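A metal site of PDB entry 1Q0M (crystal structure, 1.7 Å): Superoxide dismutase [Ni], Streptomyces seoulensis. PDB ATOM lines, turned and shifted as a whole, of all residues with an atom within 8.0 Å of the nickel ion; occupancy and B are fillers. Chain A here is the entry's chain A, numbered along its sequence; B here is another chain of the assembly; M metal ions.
A ring nitrogen (NE2) of His 1 is in hydrogen-bond range of the side-chain carboxylate (OE1) of Glu 17 of chain B (3.0 Å). A ring nitrogen (ND1) of His 1 sits at hydrogen-bond distance from the backbone carbonyl oxygen (O) of Val 8, 2.8 Å away. N of Val 8 sits close to SG of Cys 6, at 3.3 Å. SG of Cys 6 lies close to OG of Ser 20 of chain B. OG of Ser 20 of chain B lies close to ND1 of His 1 (3.4 Å). NE2 of His 1 lies within hydrogen-bond range of NH1 of Arg 47 of chain B, 3.1 Å away.
Residues that only touch the nickel ion: Asp 3 (3.7 Å). Within 4 Å of the nickel ion: His 1, Cys 2, Asp 3 and Cys 6.
The nickel ion is bound by N of Cys 2, N of His 1, SG of Cys 6 and SG of Cys 2.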
ATOM      1  N   HIS A   1      -0.571  20.170 -25.425  1.00  0.00           N
ATOM      2  CA  HIS A   1      -0.752  21.654 -25.483  1.00  0.00           C
ATOM      3  C   HIS A   1      -1.700  22.114 -24.377  1.00  0.00           C
ATOM      4  O   HIS A   1      -1.945  23.311 -24.212  1.00  0.00           O
ATOM      5  CB  HIS A   1      -1.322  22.066 -26.853  1.00  0.00           C
ATOM      6  CG  HIS A   1      -2.650  21.462 -27.173  1.00  0.00           C
ATOM      7  ND1 HIS A   1      -2.796  20.225 -27.761  1.00  0.00           N
ATOM      8  CD2 HIS A   1      -3.911  21.926 -26.977  1.00  0.00           C
ATOM      9  CE1 HIS A   1      -4.079  19.951 -27.925  1.00  0.00           C
ATOM     10  NE2 HIS A   1      -4.776  20.969 -27.453  1.00  0.00           N
ATOM     11  N   CYS A   2      -2.213  21.161 -23.622  1.00  0.00           N
ATOM     12  CA  CYS A   2      -3.142  21.413 -22.534  1.00  0.00           C
ATOM     13  C   CYS A   2      -2.458  21.518 -21.169  1.00  0.00           C
ATOM     14  O   CYS A   2      -3.118  21.757 -20.147  1.00  0.00           O
ATOM     15  CB  CYS A   2      -4.165  20.282 -22.489  1.00  0.00           C
ATOM     16  SG  CYS A   2      -3.333  18.691 -22.533  1.00  0.00           S
ATOM     17  N   ASP A   3      -1.138  21.332 -21.164  1.00  0.00           N
ATOM     18  CA  ASP A   3      -0.318  21.426 -19.948  1.00  0.00           C
ATOM     19  C   ASP A   3      -0.462  20.272 -18.955  1.00  0.00           C
ATOM     20  O   ASP A   3      -0.100  20.418 -17.790  1.00  0.00           O
ATOM     21  CB  ASP A   3      -0.618  22.750 -19.224  1.00  0.00           C
ATOM     22  CG  ASP A   3       0.636  23.385 -18.637  1.00  0.00           C
ATOM     23  OD1 ASP A   3       1.740  22.826 -18.814  1.00  0.00           O
ATOM     24  OD2 ASP A   3       0.504  24.453 -18.013  1.00  0.00           O
ATOM     25  N   LEU A   4      -0.977  19.129 -19.396  1.00  0.00           N
ATOM     26  CA  LEU A   4      -1.119  17.980 -18.494  1.00  0.00           C
ATOM     27  C   LEU A   4       0.224  17.424 -18.035  1.00  0.00           C
ATOM     28  O   LEU A   4       0.431  17.183 -16.848  1.00  0.00           O
ATOM     29  CB  LEU A   4      -1.942  16.861 -19.143  1.00  0.00           C
ATOM     30  CG  LEU A   4      -2.037  15.570 -18.295  1.00  0.00           C
ATOM     31  CD1 LEU A   4      -2.735  15.864 -16.977  1.00  0.00           C
ATOM     32  CD2 LEU A   4      -2.800  14.507 -19.070  1.00  0.00           C
ATOM     33  N   PRO A   5       1.166  17.189 -18.974  1.00  0.00           N
ATOM     34  CA  PRO A   5       1.124  17.406 -20.418  1.00  0.00           C
ATOM     35  C   PRO A   5       0.500  16.229 -21.178  1.00  0.00           C
ATOM     36  O   PRO A   5       0.526  15.093 -20.699  1.00  0.00           O
ATOM     37  CB  PRO A   5       2.596  17.591 -20.764  1.00  0.00           C
ATOM     38  CG  PRO A   5       3.233  16.583 -19.879  1.00  0.00           C
ATOM     39  CD  PRO A   5       2.526  16.800 -18.553  1.00  0.00           C
ATOM     40  N   CYS A   6      -0.032  16.504 -22.362  1.00  0.00           N
ATOM     41  CA  CYS A   6      -0.660  15.470 -23.179  1.00  0.00           C
ATOM     42  C   CYS A   6       0.266  14.960 -24.289  1.00  0.00           C
ATOM     43  O   CYS A   6       0.030  13.890 -24.856  1.00  0.00           O
ATOM     44  CB  CYS A   6      -1.945  15.989 -23.825  1.00  0.00           C
ATOM     45  SG  CYS A   6      -1.675  17.323 -25.028  1.00  0.00           S
ATOM     46  N   GLY A   7       1.301  15.732 -24.606  1.00  0.00           N
ATOM     47  CA  GLY A   7       2.234  15.324 -25.636  1.00  0.00           C
ATOM     48  C   GLY A   7       1.776  15.599 -27.061  1.00  0.00           C
ATOM     49  O   GLY A   7       2.411  15.161 -28.021  1.00  0.00           O
ATOM     50  N   VAL A   8       0.664  16.308 -27.193  1.00  0.00           N
ATOM     51  CA  VAL A   8       0.113  16.634 -28.504  1.00  0.00           C
ATOM     52  C   VAL A   8       0.254  18.137 -28.781  1.00  0.00           C
ATOM     53  O   VAL A   8      -0.336  18.964 -28.095  1.00  0.00           O
ATOM     54  CB  VAL A   8      -1.377  16.250 -28.598  1.00  0.00           C
ATOM     55  CG1 VAL A   8      -1.967  16.732 -29.916  1.00  0.00           C
ATOM     56  CG2 VAL A   8      -1.537  14.737 -28.471  1.00  0.00           C
ATOM     57  N   TYR A   9       1.043  18.458 -29.804  1.00  0.00           N
ATOM     58  CA  TYR A   9       1.268  19.847 -30.199  1.00  0.00           C
ATOM     59  C   TYR A   9       1.274  19.935 -31.708  1.00  0.00           C
ATOM     60  O   TYR A   9       1.629  18.977 -32.392  1.00  0.00           O
ATOM     61  CB  TYR A   9       2.613  20.350 -29.697  1.00  0.00           C
ATOM     62  CG  TYR A   9       2.765  20.429 -28.204  1.00  0.00           C
ATOM     63  CD1 TYR A   9       2.342  21.547 -27.499  1.00  0.00           C
ATOM     64  CD2 TYR A   9       3.369  19.394 -27.498  1.00  0.00           C
ATOM     65  CE1 TYR A   9       2.531  21.647 -26.129  1.00  0.00           C
ATOM     66  CE2 TYR A   9       3.564  19.473 -26.126  1.00  0.00           C
ATOM     67  CZ  TYR A   9       3.142  20.602 -25.452  1.00  0.00           C
ATOM     68  OH  TYR A   9       3.352  20.707 -24.093  1.00  0.00           O
ATOM     69  N   GLN A  13      -2.464  24.872 -35.221  1.00  0.00           N
ATOM     70  CA  GLN A  13      -3.503  25.552 -34.453  1.00  0.00           C
ATOM     71  C   GLN A  13      -3.308  27.052 -34.629  1.00  0.00           C
ATOM     72  O   GLN A  13      -4.254  27.787 -34.943  1.00  0.00           O
ATOM     73  CB  GLN A  13      -3.415  25.161 -32.969  1.00  0.00           C
ATOM     74  CG  GLN A  13      -3.739  23.688 -32.707  1.00  0.00           C
ATOM     75  CD  GLN A  13      -3.954  23.365 -31.235  1.00  0.00           C
ATOM     76  OE1 GLN A  13      -2.995  23.344 -30.447  1.00  0.00           O
ATOM     77  NE2 GLN A  13      -5.207  23.129 -30.860  1.00  0.00           N
ATOM     78  N   VAL A  57       1.826  29.000 -26.155  1.00  0.00           N
ATOM     79  CA  VAL A  57       1.847  27.642 -25.631  1.00  0.00           C
ATOM     80  C   VAL A  57       3.037  26.843 -26.162  1.00  0.00           C
ATOM     81  O   VAL A  57       3.681  26.104 -25.418  1.00  0.00           O
ATOM     82  CB  VAL A  57       0.532  26.893 -25.974  1.00  0.00           C
ATOM     83  CG1 VAL A  57       0.667  25.393 -25.684  1.00  0.00           C
ATOM     84  CG2 VAL A  57      -0.601  27.475 -25.146  1.00  0.00           C
ATOM     85  N   ASP A  61       5.323  25.790 -23.201  1.00  0.00           N
ATOM     86  CA  ASP A  61       5.170  24.360 -22.902  1.00  0.00           C
ATOM     87  C   ASP A  61       5.950  23.363 -23.748  1.00  0.00           C
ATOM     88  O   ASP A  61       6.579  22.460 -23.197  1.00  0.00           O
ATOM     89  CB  ASP A  61       3.694  23.995 -22.958  1.00  0.00           C
ATOM     90  CG  ASP A  61       2.858  24.750 -21.935  1.00  0.00           C
ATOM     91  OD1 ASP A  61       3.367  25.712 -21.332  1.00  0.00           O
ATOM     92  OD2 ASP A  61       1.682  24.371 -21.745  1.00  0.00           O
ATOM     93  N   ILE B  16      -7.273  17.665 -33.652  1.00  0.00           N
ATOM     94  CA  ILE B  16      -6.172  17.828 -32.723  1.00  0.00           C
ATOM     95  C   ILE B  16      -6.644  17.742 -31.279  1.00  0.00           C
ATOM     96  O   ILE B  16      -5.972  17.142 -30.430  1.00  0.00           O
ATOM     97  CB  ILE B  16      -5.412  19.157 -32.943  1.00  0.00           C
ATOM     98  CG1 ILE B  16      -4.129  19.150 -32.103  1.00  0.00           C
ATOM     99  CG2 ILE B  16      -6.283  20.345 -32.573  1.00  0.00           C
ATOM    100  CD1 ILE B  16      -3.195  20.305 -32.393  1.00  0.00           C
ATOM    101  N   GLU B  17      -7.799  18.335 -30.986  1.00  0.00           N
ATOM    102  CA  GLU B  17      -8.312  18.282 -29.627  1.00  0.00           C
ATOM    103  C   GLU B  17      -8.728  16.855 -29.281  1.00  0.00           C
ATOM    104  O   GLU B  17      -8.509  16.407 -28.162  1.00  0.00           O
ATOM    105  CB  GLU B  17      -9.494  19.254 -29.458  1.00  0.00           C
ATOM    106  CG  GLU B  17      -9.123  20.735 -29.579  1.00  0.00           C
ATOM    107  CD  GLU B  17      -7.997  21.164 -28.628  1.00  0.00           C
ATOM    108  OE1 GLU B  17      -7.717  20.435 -27.658  1.00  0.00           O
ATOM    109  OE2 GLU B  17      -7.397  22.237 -28.862  1.00  0.00           O
ATOM    110  N   SER B  20      -5.788  14.785 -28.373  1.00  0.00           N
ATOM    111  CA  SER B  20      -5.321  15.030 -27.006  1.00  0.00           C
ATOM    112  C   SER B  20      -6.173  14.219 -26.049  1.00  0.00           C
ATOM    113  O   SER B  20      -5.664  13.657 -25.075  1.00  0.00           O
ATOM    114  CB  SER B  20      -5.429  16.523 -26.651  1.00  0.00           C
ATOM    115  OG  SER B  20      -4.433  17.256 -27.326  1.00  0.00           O
ATOM    116  N   VAL B  21      -7.472  14.154 -26.318  1.00  0.00           N
ATOM    117  CA  VAL B  21      -8.379  13.388 -25.478  1.00  0.00           C
ATOM    118  C   VAL B  21      -7.908  11.937 -25.401  1.00  0.00           C
ATOM    119  O   VAL B  21      -7.775  11.389 -24.301  1.00  0.00           O
ATOM    120  CB  VAL B  21      -9.821  13.432 -26.012  1.00  0.00           C
ATOM    121  CG1 VAL B  21     -10.688  12.426 -25.275  1.00  0.00           C
ATOM    122  CG2 VAL B  21     -10.396  14.844 -25.814  1.00  0.00           C
ATOM    123  N   ALA B  23      -4.932  10.736 -26.139  1.00  0.00           N
ATOM    124  CA  ALA B  23      -3.590  10.699 -25.566  1.00  0.00           C
ATOM    125  C   ALA B  23      -3.658  10.764 -24.044  1.00  0.00           C
ATOM    126  O   ALA B  23      -2.914  10.075 -23.345  1.00  0.00           O
ATOM    127  CB  ALA B  23      -2.758  11.863 -26.100  1.00  0.00           C
ATOM    128  N   ILE B  24      -4.549  11.611 -23.535  1.00  0.00           N
ATOM    129  CA  ILE B  24      -4.707  11.747 -22.093  1.00  0.00           C
ATOM    130  C   ILE B  24      -5.237  10.434 -21.509  1.00  0.00           C
ATOM    131  O   ILE B  24      -4.799   9.982 -20.448  1.00  0.00           O
ATOM    132  CB  ILE B  24      -5.676  12.905 -21.751  1.00  0.00           C
ATOM    133  CG1 ILE B  24      -5.035  14.235 -22.164  1.00  0.00           C
ATOM    134  CG2 ILE B  24      -5.985  12.912 -20.266  1.00  0.00           C
ATOM    135  CD1 ILE B  24      -5.965  15.446 -22.038  1.00  0.00           C
ATOM    136  N   LYS B  27      -2.457   8.054 -21.172  1.00  0.00           N
ATOM    137  CA  LYS B  27      -1.604   8.366 -20.030  1.00  0.00           C
ATOM    138  C   LYS B  27      -2.257   7.993 -18.697  1.00  0.00           C
ATOM    139  O   LYS B  27      -1.568   7.617 -17.752  1.00  0.00           O
ATOM    140  CB  LYS B  27      -1.241   9.854 -20.031  1.00  0.00           C
ATOM    141  CG  LYS B  27      -0.336  10.244 -21.182  1.00  0.00           C
ATOM    142  CD  LYS B  27       0.040  11.709 -21.130  1.00  0.00           C
ATOM    143  CE  LYS B  27       0.909  12.074 -22.319  1.00  0.00           C
ATOM    144  NZ  LYS B  27       2.135  11.228 -22.371  1.00  0.00           N
ATOM    145  N   ILE B  43      -8.500  18.133 -17.487  1.00  0.00           N
ATOM    146  CA  ILE B  43      -7.996  18.534 -18.794  1.00  0.00           C
ATOM    147  C   ILE B  43      -8.671  17.790 -19.946  1.00  0.00           C
ATOM    148  O   ILE B  43      -8.945  18.390 -20.992  1.00  0.00           O
ATOM    149  CB  ILE B  43      -6.463  18.352 -18.847  1.00  0.00           C
ATOM    150  CG1 ILE B  43      -5.817  19.326 -17.862  1.00  0.00           C
ATOM    151  CG2 ILE B  43      -5.960  18.569 -20.265  1.00  0.00           C
ATOM    152  CD1 ILE B  43      -4.306  19.213 -17.752  1.00  0.00           C
ATOM    153  N   ARG B  47     -10.547  19.528 -23.211  1.00  0.00           N
ATOM    154  CA  ARG B  47     -10.180  19.254 -24.595  1.00  0.00           C
ATOM    155  C   ARG B  47     -11.352  18.673 -25.388  1.00  0.00           C
ATOM    156  O   ARG B  47     -11.565  19.024 -26.547  1.00  0.00           O
ATOM    157  CB  ARG B  47      -8.984  18.308 -24.657  1.00  0.00           C
ATOM    158  CG  ARG B  47      -7.695  18.891 -24.084  1.00  0.00           C
ATOM    159  CD  ARG B  47      -7.270  20.119 -24.870  1.00  0.00           C
ATOM    160  NE  ARG B  47      -7.304  21.322 -24.049  1.00  0.00           N
ATOM    161  CZ  ARG B  47      -7.017  22.542 -24.485  1.00  0.00           C
ATOM    162  NH1 ARG B  47      -6.694  22.744 -25.751  1.00  0.00           N
ATOM    163  NH2 ARG B  47      -7.055  23.562 -23.643  1.00  0.00           N
HETATM  164 NI    NI M   1      -1.903  19.301 -24.115  1.00  0.00          NI
